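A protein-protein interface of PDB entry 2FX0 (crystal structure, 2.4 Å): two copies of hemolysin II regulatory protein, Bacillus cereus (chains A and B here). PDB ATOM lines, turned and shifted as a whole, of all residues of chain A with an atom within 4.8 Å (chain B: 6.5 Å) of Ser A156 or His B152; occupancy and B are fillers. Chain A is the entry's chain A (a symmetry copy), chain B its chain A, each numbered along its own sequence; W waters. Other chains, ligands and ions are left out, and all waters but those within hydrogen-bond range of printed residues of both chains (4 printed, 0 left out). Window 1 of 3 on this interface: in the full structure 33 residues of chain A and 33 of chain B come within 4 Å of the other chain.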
ATOM      1  N   HIS A 152      20.969  -9.319  -5.302  1.00  0.00           N
ATOM      2  CA  HIS A 152      19.728  -8.884  -4.641  1.00  0.00           C
ATOM      3  C   HIS A 152      18.493  -9.092  -5.533  1.00  0.00           C
ATOM      4  O   HIS A 152      17.616  -9.889  -5.168  1.00  0.00           O
ATOM      5  CB  HIS A 152      19.808  -7.416  -4.223  1.00  0.00           C
ATOM      6  CG  HIS A 152      20.332  -7.195  -2.839  1.00  0.00           C
ATOM      7  ND1 HIS A 152      19.504  -7.064  -1.742  1.00  0.00           N
ATOM      8  CD2 HIS A 152      21.594  -7.042  -2.379  1.00  0.00           C
ATOM      9  CE1 HIS A 152      20.238  -6.857  -0.663  1.00  0.00           C
ATOM     10  NE2 HIS A 152      21.509  -6.843  -1.023  1.00  0.00           N
ATOM     11  N   TRP A 153      18.443  -8.419  -6.699  1.00  0.00           N
ATOM     12  CA  TRP A 153      17.227  -8.409  -7.545  1.00  0.00           C
ATOM     13  C   TRP A 153      16.923  -9.697  -8.283  1.00  0.00           C
ATOM     14  O   TRP A 153      15.760  -9.967  -8.588  1.00  0.00           O
ATOM     15  CB  TRP A 153      17.111  -7.172  -8.493  1.00  0.00           C
ATOM     16  CG  TRP A 153      17.931  -7.152  -9.780  1.00  0.00           C
ATOM     17  CD1 TRP A 153      19.049  -6.397 -10.021  1.00  0.00           C
ATOM     18  CD2 TRP A 153      17.669  -7.875 -11.011  1.00  0.00           C
ATOM     19  NE1 TRP A 153      19.516  -6.624 -11.308  1.00  0.00           N
ATOM     20  CE2 TRP A 153      18.696  -7.523 -11.933  1.00  0.00           C
ATOM     21  CE3 TRP A 153      16.681  -8.797 -11.415  1.00  0.00           C
ATOM     22  CZ2 TRP A 153      18.769  -8.066 -13.231  1.00  0.00           C
ATOM     23  CZ3 TRP A 153      16.756  -9.336 -12.714  1.00  0.00           C
ATOM     24  CH2 TRP A 153      17.795  -8.963 -13.604  1.00  0.00           C
ATOM     25  N   ILE A 154      17.941 -10.500  -8.574  1.00  0.00           N
ATOM     26  CA  ILE A 154      17.690 -11.770  -9.245  1.00  0.00           C
ATOM     27  C   ILE A 154      17.010 -12.679  -8.238  1.00  0.00           C
ATOM     28  O   ILE A 154      15.974 -13.258  -8.533  1.00  0.00           O
ATOM     29  CB  ILE A 154      18.966 -12.419  -9.841  1.00  0.00           C
ATOM     30  CG1 ILE A 154      19.460 -11.606 -11.039  1.00  0.00           C
ATOM     31  CG2 ILE A 154      18.664 -13.852 -10.285  1.00  0.00           C
ATOM     32  CD1 ILE A 154      20.827 -12.037 -11.608  1.00  0.00           C
ATOM     33  N   THR A 155      17.599 -12.770  -7.048  1.00  0.00           N
ATOM     34  CA  THR A 155      17.045 -13.528  -5.912  1.00  0.00           C
ATOM     35  C   THR A 155      15.570 -13.217  -5.651  1.00  0.00           C
ATOM     36  O   THR A 155      14.721 -14.113  -5.673  1.00  0.00           O
ATOM     37  CB  THR A 155      17.859 -13.253  -4.629  1.00  0.00           C
ATOM     38  OG1 THR A 155      19.242 -13.525  -4.888  1.00  0.00           O
ATOM     39  CG2 THR A 155      17.389 -14.133  -3.491  1.00  0.00           C
ATOM     40  N   SER A 156      15.281 -11.938  -5.428  1.00  0.00           N
ATOM     41  CA  SER A 156      13.922 -11.482  -5.149  1.00  0.00           C
ATOM     42  C   SER A 156      12.895 -11.935  -6.191  1.00  0.00           C
ATOM     43  O   SER A 156      11.879 -12.528  -5.818  1.00  0.00           O
ATOM     44  CB  SER A 156      13.886  -9.967  -4.981  1.00  0.00           C
ATOM     45  OG  SER A 156      12.569  -9.520  -4.683  1.00  0.00           O
ATOM     46  N   ILE A 157      13.161 -11.698  -7.484  1.00  0.00           N
ATOM     47  CA  ILE A 157      12.163 -12.004  -8.518  1.00  0.00           C
ATOM     48  C   ILE A 157      12.018 -13.492  -8.822  1.00  0.00           C
ATOM     49  O   ILE A 157      11.033 -13.917  -9.435  1.00  0.00           O
ATOM     50  CB  ILE A 157      12.369 -11.191  -9.830  1.00  0.00           C
ATOM     51  CG1 ILE A 157      11.002 -10.935 -10.488  1.00  0.00           C
ATOM     52  CG2 ILE A 157      13.409 -11.878 -10.773  1.00  0.00           C
ATOM     53  CD1 ILE A 157      11.039 -10.505 -11.970  1.00  0.00           C
ATOM     54  N   VAL A 158      12.999 -14.277  -8.387  1.00  0.00           N
ATOM     55  CA  VAL A 158      12.996 -15.722  -8.591  1.00  0.00           C
ATOM     56  C   VAL A 158      12.285 -16.395  -7.415  1.00  0.00           C
ATOM     57  O   VAL A 158      11.400 -17.239  -7.608  1.00  0.00           O
ATOM     58  CB  VAL A 158      14.449 -16.262  -8.752  1.00  0.00           C
ATOM     59  CG1 VAL A 158      14.486 -17.787  -8.702  1.00  0.00           C
ATOM     60  CG2 VAL A 158      15.066 -15.756 -10.053  1.00  0.00           C
ATOM     61  N   LEU A 159      12.676 -16.005  -6.201  1.00  0.00           N
ATOM     62  CA  LEU A 159      12.097 -16.548  -4.969  1.00  0.00           C
ATOM     63  C   LEU A 159      10.654 -16.141  -4.788  1.00  0.00           C
ATOM     64  O   LEU A 159       9.837 -16.930  -4.320  1.00  0.00           O
ATOM     65  CB  LEU A 159      12.898 -16.094  -3.748  1.00  0.00           C
ATOM     66  CG  LEU A 159      14.154 -16.898  -3.393  1.00  0.00           C
ATOM     67  CD1 LEU A 159      14.875 -16.274  -2.217  1.00  0.00           C
ATOM     68  CD2 LEU A 159      13.816 -18.352  -3.080  1.00  0.00           C
ATOM     69  N   PHE A 160      10.346 -14.904  -5.176  1.00  0.00           N
ATOM     70  CA  PHE A 160       9.055 -14.290  -4.876  1.00  0.00           C
ATOM     71  C   PHE A 160       8.320 -13.801  -6.146  1.00  0.00           C
ATOM     72  O   PHE A 160       8.376 -12.611  -6.479  1.00  0.00           O
ATOM     73  CB  PHE A 160       9.248 -13.178  -3.831  1.00  0.00           C
ATOM     74  CG  PHE A 160      10.143 -13.586  -2.668  1.00  0.00           C
ATOM     75  CD1 PHE A 160       9.737 -14.567  -1.760  1.00  0.00           C
ATOM     76  CD2 PHE A 160      11.393 -13.002  -2.491  1.00  0.00           C
ATOM     77  CE1 PHE A 160      10.571 -14.957  -0.690  1.00  0.00           C
ATOM     78  CE2 PHE A 160      12.224 -13.380  -1.426  1.00  0.00           C
ATOM     79  CZ  PHE A 160      11.812 -14.363  -0.525  1.00  0.00           C
ATOM     80  N   PHE A 163       5.408 -11.202  -5.543  1.00  0.00           N
ATOM     81  CA  PHE A 163       5.909  -9.839  -5.393  1.00  0.00           C
ATOM     82  C   PHE A 163       6.240  -9.250  -6.740  1.00  0.00           C
ATOM     83  O   PHE A 163       6.174  -8.025  -6.912  1.00  0.00           O
ATOM     84  CB  PHE A 163       7.141  -9.801  -4.492  1.00  0.00           C
ATOM     85  CG  PHE A 163       7.693  -8.416  -4.268  1.00  0.00           C
ATOM     86  CD1 PHE A 163       6.909  -7.413  -3.716  1.00  0.00           C
ATOM     87  CD2 PHE A 163       9.005  -8.126  -4.572  1.00  0.00           C
ATOM     88  CE1 PHE A 163       7.426  -6.150  -3.488  1.00  0.00           C
ATOM     89  CE2 PHE A 163       9.515  -6.857  -4.353  1.00  0.00           C
ATOM     90  CZ  PHE A 163       8.728  -5.875  -3.809  1.00  0.00           C
ATOM     91  N   LYS A 164       6.605 -10.121  -7.690  1.00  0.00           N
ATOM     92  CA  LYS A 164       6.799  -9.705  -9.073  1.00  0.00           C
ATOM     93  C   LYS A 164       5.502  -9.110  -9.605  1.00  0.00           C
ATOM     94  O   LYS A 164       5.508  -8.024 -10.195  1.00  0.00           O
ATOM     95  CB  LYS A 164       7.248 -10.877  -9.956  1.00  0.00           C
ATOM     96  CG  LYS A 164       7.238 -10.564 -11.449  1.00  0.00           C
ATOM     97  CD  LYS A 164       7.107 -11.825 -12.274  1.00  0.00           C
ATOM     98  CE  LYS A 164       6.348 -11.566 -13.567  1.00  0.00           C
ATOM     99  NZ  LYS A 164       6.208 -12.800 -14.388  1.00  0.00           N
ATOM    100  N   ILE A 167       4.548  -5.683  -8.119  1.00  0.00           N
ATOM    101  CA  ILE A 167       5.329  -4.648  -8.790  1.00  0.00           C
ATOM    102  C   ILE A 167       4.782  -4.424 -10.191  1.00  0.00           C
ATOM    103  O   ILE A 167       4.187  -3.371 -10.471  1.00  0.00           O
ATOM    104  CB  ILE A 167       6.846  -4.997  -8.839  1.00  0.00           C
ATOM    105  CG1 ILE A 167       7.447  -5.099  -7.425  1.00  0.00           C
ATOM    106  CG2 ILE A 167       7.605  -3.982  -9.670  1.00  0.00           C
ATOM    107  CD1 ILE A 167       7.231  -3.866  -6.546  1.00  0.00           C
ATOM    108  N   ILE B 109       5.967  -9.575   0.217  1.00  0.00           N
ATOM    109  CA  ILE B 109       7.008 -10.273  -0.533  1.00  0.00           C
ATOM    110  C   ILE B 109       6.681 -11.747  -0.765  1.00  0.00           C
ATOM    111  O   ILE B 109       6.390 -12.145  -1.887  1.00  0.00           O
ATOM    112  CB  ILE B 109       8.455  -9.929  -0.004  1.00  0.00           C
ATOM    113  CG1 ILE B 109       8.832  -8.505  -0.475  1.00  0.00           C
ATOM    114  CG2 ILE B 109       9.497 -10.901  -0.540  1.00  0.00           C
ATOM    115  CD1 ILE B 109       9.874  -7.757   0.369  1.00  0.00           C
ATOM    116  N   LEU B 129       7.657   5.976  -4.162  1.00  0.00           N
ATOM    117  CA  LEU B 129       8.985   5.616  -4.643  1.00  0.00           C
ATOM    118  C   LEU B 129       9.023   5.548  -6.173  1.00  0.00           C
ATOM    119  O   LEU B 129       9.982   6.025  -6.809  1.00  0.00           O
ATOM    120  CB  LEU B 129       9.458   4.281  -4.048  1.00  0.00           C
ATOM    121  CG  LEU B 129      10.758   3.745  -4.673  1.00  0.00           C
ATOM    122  CD1 LEU B 129      11.994   4.592  -4.287  1.00  0.00           C
ATOM    123  CD2 LEU B 129      11.004   2.276  -4.387  1.00  0.00           C
ATOM    124  N   ILE B 147      12.400  -0.162 -14.265  1.00  0.00           N
ATOM    125  CA  ILE B 147      11.876   0.486 -13.071  1.00  0.00           C
ATOM    126  C   ILE B 147      11.546  -0.584 -12.017  1.00  0.00           C
ATOM    127  O   ILE B 147      11.874  -0.425 -10.840  1.00  0.00           O
ATOM    128  CB  ILE B 147      10.693   1.443 -13.402  1.00  0.00           C
ATOM    129  CG1 ILE B 147       9.987   1.924 -12.121  1.00  0.00           C
ATOM    130  CG2 ILE B 147       9.697   0.792 -14.363  1.00  0.00           C
ATOM    131  CD1 ILE B 147      10.693   3.059 -11.385  1.00  0.00           C
ATOM    132  N   ASN B 148      10.972  -1.703 -12.465  1.00  0.00           N
ATOM    133  CA  ASN B 148      10.650  -2.839 -11.596  1.00  0.00           C
ATOM    134  C   ASN B 148      11.814  -3.414 -10.779  1.00  0.00           C
ATOM    135  O   ASN B 148      11.684  -3.587  -9.554  1.00  0.00           O
ATOM    136  CB  ASN B 148       9.992  -3.958 -12.404  1.00  0.00           C
ATOM    137  CG  ASN B 148       8.660  -3.543 -12.987  1.00  0.00           C
ATOM    138  OD1 ASN B 148       8.165  -2.448 -12.723  1.00  0.00           O
ATOM    139  ND2 ASN B 148       8.071  -4.417 -13.787  1.00  0.00           N
ATOM    140  N   HIS B 149      12.934  -3.729 -11.442  1.00  0.00           N
ATOM    141  CA  HIS B 149      14.083  -4.317 -10.741  1.00  0.00           C
ATOM    142  C   HIS B 149      14.633  -3.323  -9.740  1.00  0.00           C
ATOM    143  O   HIS B 149      15.034  -3.709  -8.635  1.00  0.00           O
ATOM    144  CB  HIS B 149      15.205  -4.732 -11.704  1.00  0.00           C
ATOM    145  CG  HIS B 149      14.786  -5.722 -12.746  1.00  0.00           C
ATOM    146  ND1 HIS B 149      13.657  -6.507 -12.625  1.00  0.00           N
ATOM    147  CD2 HIS B 149      15.363  -6.071 -13.919  1.00  0.00           C
ATOM    148  CE1 HIS B 149      13.546  -7.282 -13.690  1.00  0.00           C
ATOM    149  NE2 HIS B 149      14.568  -7.036 -14.491  1.00  0.00           N
ATOM    150  N   THR B 150      14.645  -2.041 -10.151  1.00  0.00           N
ATOM    151  CA  THR B 150      15.116  -0.938  -9.318  1.00  0.00           C
ATOM    152  C   THR B 150      14.270  -0.798  -8.062  1.00  0.00           C
ATOM    153  O   THR B 150      14.792  -0.555  -6.967  1.00  0.00           O
ATOM    154  CB  THR B 150      15.100   0.411 -10.074  1.00  0.00           C
ATOM    155  OG1 THR B 150      15.882   0.309 -11.272  1.00  0.00           O
ATOM    156  CG2 THR B 150      15.677   1.488  -9.201  1.00  0.00           C
ATOM    157  N   ILE B 151      12.956  -0.918  -8.241  1.00  0.00           N
ATOM    158  CA  ILE B 151      12.039  -0.945  -7.115  1.00  0.00           C
ATOM    159  C   ILE B 151      12.335  -2.182  -6.267  1.00  0.00           C
ATOM    160  O   ILE B 151      12.567  -2.061  -5.053  1.00  0.00           O
ATOM    161  CB  ILE B 151      10.570  -0.907  -7.574  1.00  0.00           C
ATOM    162  CG1 ILE B 151      10.261   0.485  -8.165  1.00  0.00           C
ATOM    163  CG2 ILE B 151       9.659  -1.243  -6.402  1.00  0.00           C
ATOM    164  CD1 ILE B 151       8.896   0.629  -8.829  1.00  0.00           C
ATOM    165  N   HIS B 152      12.369  -3.351  -6.917  1.00  0.00           N
ATOM    166  CA  HIS B 152      12.800  -4.598  -6.266  1.00  0.00           C
ATOM    167  C   HIS B 152      14.035  -4.388  -5.374  1.00  0.00           C
ATOM    168  O   HIS B 152      13.933  -4.573  -4.153  1.00  0.00           O
ATOM    169  CB  HIS B 152      13.098  -5.687  -7.295  1.00  0.00           C
ATOM    170  CG  HIS B 152      11.926  -6.556  -7.631  1.00  0.00           C
ATOM    171  ND1 HIS B 152      11.686  -7.758  -6.996  1.00  0.00           N
ATOM    172  CD2 HIS B 152      10.954  -6.419  -8.560  1.00  0.00           C
ATOM    173  CE1 HIS B 152      10.603  -8.315  -7.509  1.00  0.00           C
ATOM    174  NE2 HIS B 152      10.139  -7.521  -8.458  1.00  0.00           N
ATOM    175  N   TRP B 153      15.172  -3.973  -5.969  1.00  0.00           N
ATOM    176  CA  TRP B 153      16.459  -3.912  -5.238  1.00  0.00           C
ATOM    177  C   TRP B 153      16.590  -2.796  -4.221  1.00  0.00           C
ATOM    178  O   TRP B 153      17.348  -2.933  -3.258  1.00  0.00           O
ATOM    179  CB  TRP B 153      17.724  -3.997  -6.152  1.00  0.00           C
ATOM    180  CG  TRP B 153      18.168  -2.751  -6.912  1.00  0.00           C
ATOM    181  CD1 TRP B 153      18.028  -2.526  -8.257  1.00  0.00           C
ATOM    182  CD2 TRP B 153      18.865  -1.592  -6.386  1.00  0.00           C
ATOM    183  NE1 TRP B 153      18.565  -1.293  -8.598  1.00  0.00           N
ATOM    184  CE2 TRP B 153      19.080  -0.699  -7.477  1.00  0.00           C
ATOM    185  CE3 TRP B 153      19.311  -1.214  -5.104  1.00  0.00           C
ATOM    186  CZ2 TRP B 153      19.712   0.550  -7.322  1.00  0.00           C
ATOM    187  CZ3 TRP B 153      19.944   0.035  -4.952  1.00  0.00           C
ATOM    188  CH2 TRP B 153      20.138   0.897  -6.060  1.00  0.00           C
ATOM    189  N   ILE B 154      15.869  -1.697  -4.410  1.00  0.00           N
ATOM    190  CA  ILE B 154      15.931  -0.616  -3.433  1.00  0.00           C
ATOM    191  C   ILE B 154      15.219  -1.102  -2.184  1.00  0.00           C
ATOM    192  O   ILE B 154      15.763  -1.016  -1.092  1.00  0.00           O
ATOM    193  CB  ILE B 154      15.342   0.722  -3.950  1.00  0.00           C
ATOM    194  CG1 ILE B 154      16.252   1.316  -5.027  1.00  0.00           C
ATOM    195  CG2 ILE B 154      15.205   1.714  -2.794  1.00  0.00           C
ATOM    196  CD1 ILE B 154      15.688   2.551  -5.759  1.00  0.00           C
ATOM    197  N   THR B 155      14.012  -1.630  -2.372  1.00  0.00           N
ATOM    198  CA  THR B 155      13.203  -2.238  -1.301  1.00  0.00           C
ATOM    199  C   THR B 155      13.993  -3.236  -0.451  1.00  0.00           C
ATOM    200  O   THR B 155      14.103  -3.080   0.768  1.00  0.00           O
ATOM    201  CB  THR B 155      11.962  -2.941  -1.892  1.00  0.00           C
ATOM    202  OG1 THR B 155      11.240  -2.007  -2.703  1.00  0.00           O
ATOM    203  CG2 THR B 155      11.051  -3.444  -0.792  1.00  0.00           C
ATOM    204  N   SER B 156      14.556  -4.241  -1.116  1.00  0.00           N
ATOM    205  CA  SER B 156      15.329  -5.284  -0.448  1.00  0.00           C
ATOM    206  C   SER B 156      16.446  -4.740   0.449  1.00  0.00           C
ATOM    207  O   SER B 156      16.505  -5.106   1.626  1.00  0.00           O
ATOM    208  CB  SER B 156      15.887  -6.275  -1.462  1.00  0.00           C
ATOM    209  OG  SER B 156      16.621  -7.306  -0.814  1.00  0.00           O
ATOM    210  N   ILE B 157      17.303  -3.852  -0.077  1.00  0.00           N
ATOM    211  CA  ILE B 157      18.460  -3.386   0.697  1.00  0.00           C
ATOM    212  C   ILE B 157      18.111  -2.393   1.802  1.00  0.00           C
ATOM    213  O   ILE B 157      18.916  -2.148   2.708  1.00  0.00           O
ATOM    214  CB  ILE B 157      19.613  -2.837  -0.192  1.00  0.00           C
ATOM    215  CG1 ILE B 157      20.962  -3.112   0.496  1.00  0.00           C
ATOM    216  CG2 ILE B 157      19.386  -1.336  -0.566  1.00  0.00           C
ATOM    217  CD1 ILE B 157      22.164  -2.300  -0.030  1.00  0.00           C
HETATM  218  O   HOH W   1      16.868  -9.605  -2.488  1.00  0.00           O
HETATM  219  O   HOH W   2       8.245  -7.302 -11.117  1.00  0.00           O
HETATM  220  O   HOH W   3       6.290  -1.176 -11.596  1.00  0.00           O
HETATM  221  O   HOH W   4      12.605  -6.937  -3.469  1.00  0.00           O
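ND1 of His B152 sits at hydrogen-bond distance from OG of Ser A156. The side-chain hydroxyl of Ser B156 sits at hydrogen-bond distance from a ring nitrogen (ND1) of His A152, at 3.0 Å.
The side-chain hydroxyl (OG1) of Thr B155 is in hydrogen-bond range of the backbone carbonyl oxygen (O) of Ile B151 (2.7 Å).
Among the printed residues, merely in contact across the chains: Phe A163 with His B152 (3.3 Å), Phe A160 with Ile B109 (3.4 Å), Ile A167 with Asn B148 (3.5 Å), Ile A167 with Ile B151 (3.6 Å), Phe A163 with Ile B109 (3.6 Å), Trp A153 with His B149 (3.6 Å), Ile A167 with His B152 (3.8 Å), His A152 with Ile B157 (3.99 Å), Ile A157 with His B152 (3.99 Å) and Trp A153 with Trp B153 (3.99 Å).
Of chain B, only His B152 comes within 4 Å of Ser A156. Of the printed residues of chain A, His B152 touches Ser A156 (3.0 Å), Ile A157 (3.99 Å), Phe A163 (3.3 Å) and Ile A167 (3.8 Å). Of the printed residues of chain A, Ile B157 touches His A152. Of the printed residues of chain A, Ile B151 touches Ile A167 (3.6 Å). Of the printed residues of chain A, Ser B156 touches His A152. The nearest printed residue of chain A that does not touch His B152 is Lys A164 (4.04 Å).
Of the 12 printed residues of chain A, 7 touch a printed residue of chain B. Hydrophobic or aromatic side chains of chain A within 4 Å of the printed part of chain B: His A152, Trp A153, Ile A157, Phe A160, Phe A163 and Ile A167. Along chain A the printed residues that touch a printed residue of chain B span positions 152 to 167. Of the 13 printed residues of chain B, 8 touch a printed residue of chain A. Hydrophobic or aromatic side chains of chain B within 4 Å of the printed part of chain A: Ile B109, His B149, Ile B151, His B152, Trp B153 and Ile B157. Among the printed residues, no Asp or Glu carboxylate lies within 4 Å of a Lys or Arg side-chain nitrogen of the other chain.
His A152 touches Ser B156, and with the chains exchanged Ser A156 touches His B152. His A152 touches Ile B157, and with the chains exchanged Ile A157 touches His B152. Trp B153 touches its own counterpart, Trp A153. 6 positions are printed for both chains. Of the 12 pairs that touch across the chains among the printed residues, 5 have their exchanged pair printed and touching as well.
Water W3 bridges the side-chain amide oxygen (OD1) of Asn B148 and the backbone carbonyl oxygen (O) of Ile A167. Water W4 lies within hydrogen-bond range of O of His B152 (2.8 Å) and OG of Ser A156 (2.9 Å). Water W1 bridges O of His A152 (2.8 Å) and OG of Ser B156 (2.9 Å). Water W2 lies within hydrogen-bond range of the backbone carbonyl oxygen (O) of Lys A164 (3.0 Å) and a ring nitrogen (NE2) of His B152 (3.3 Å).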
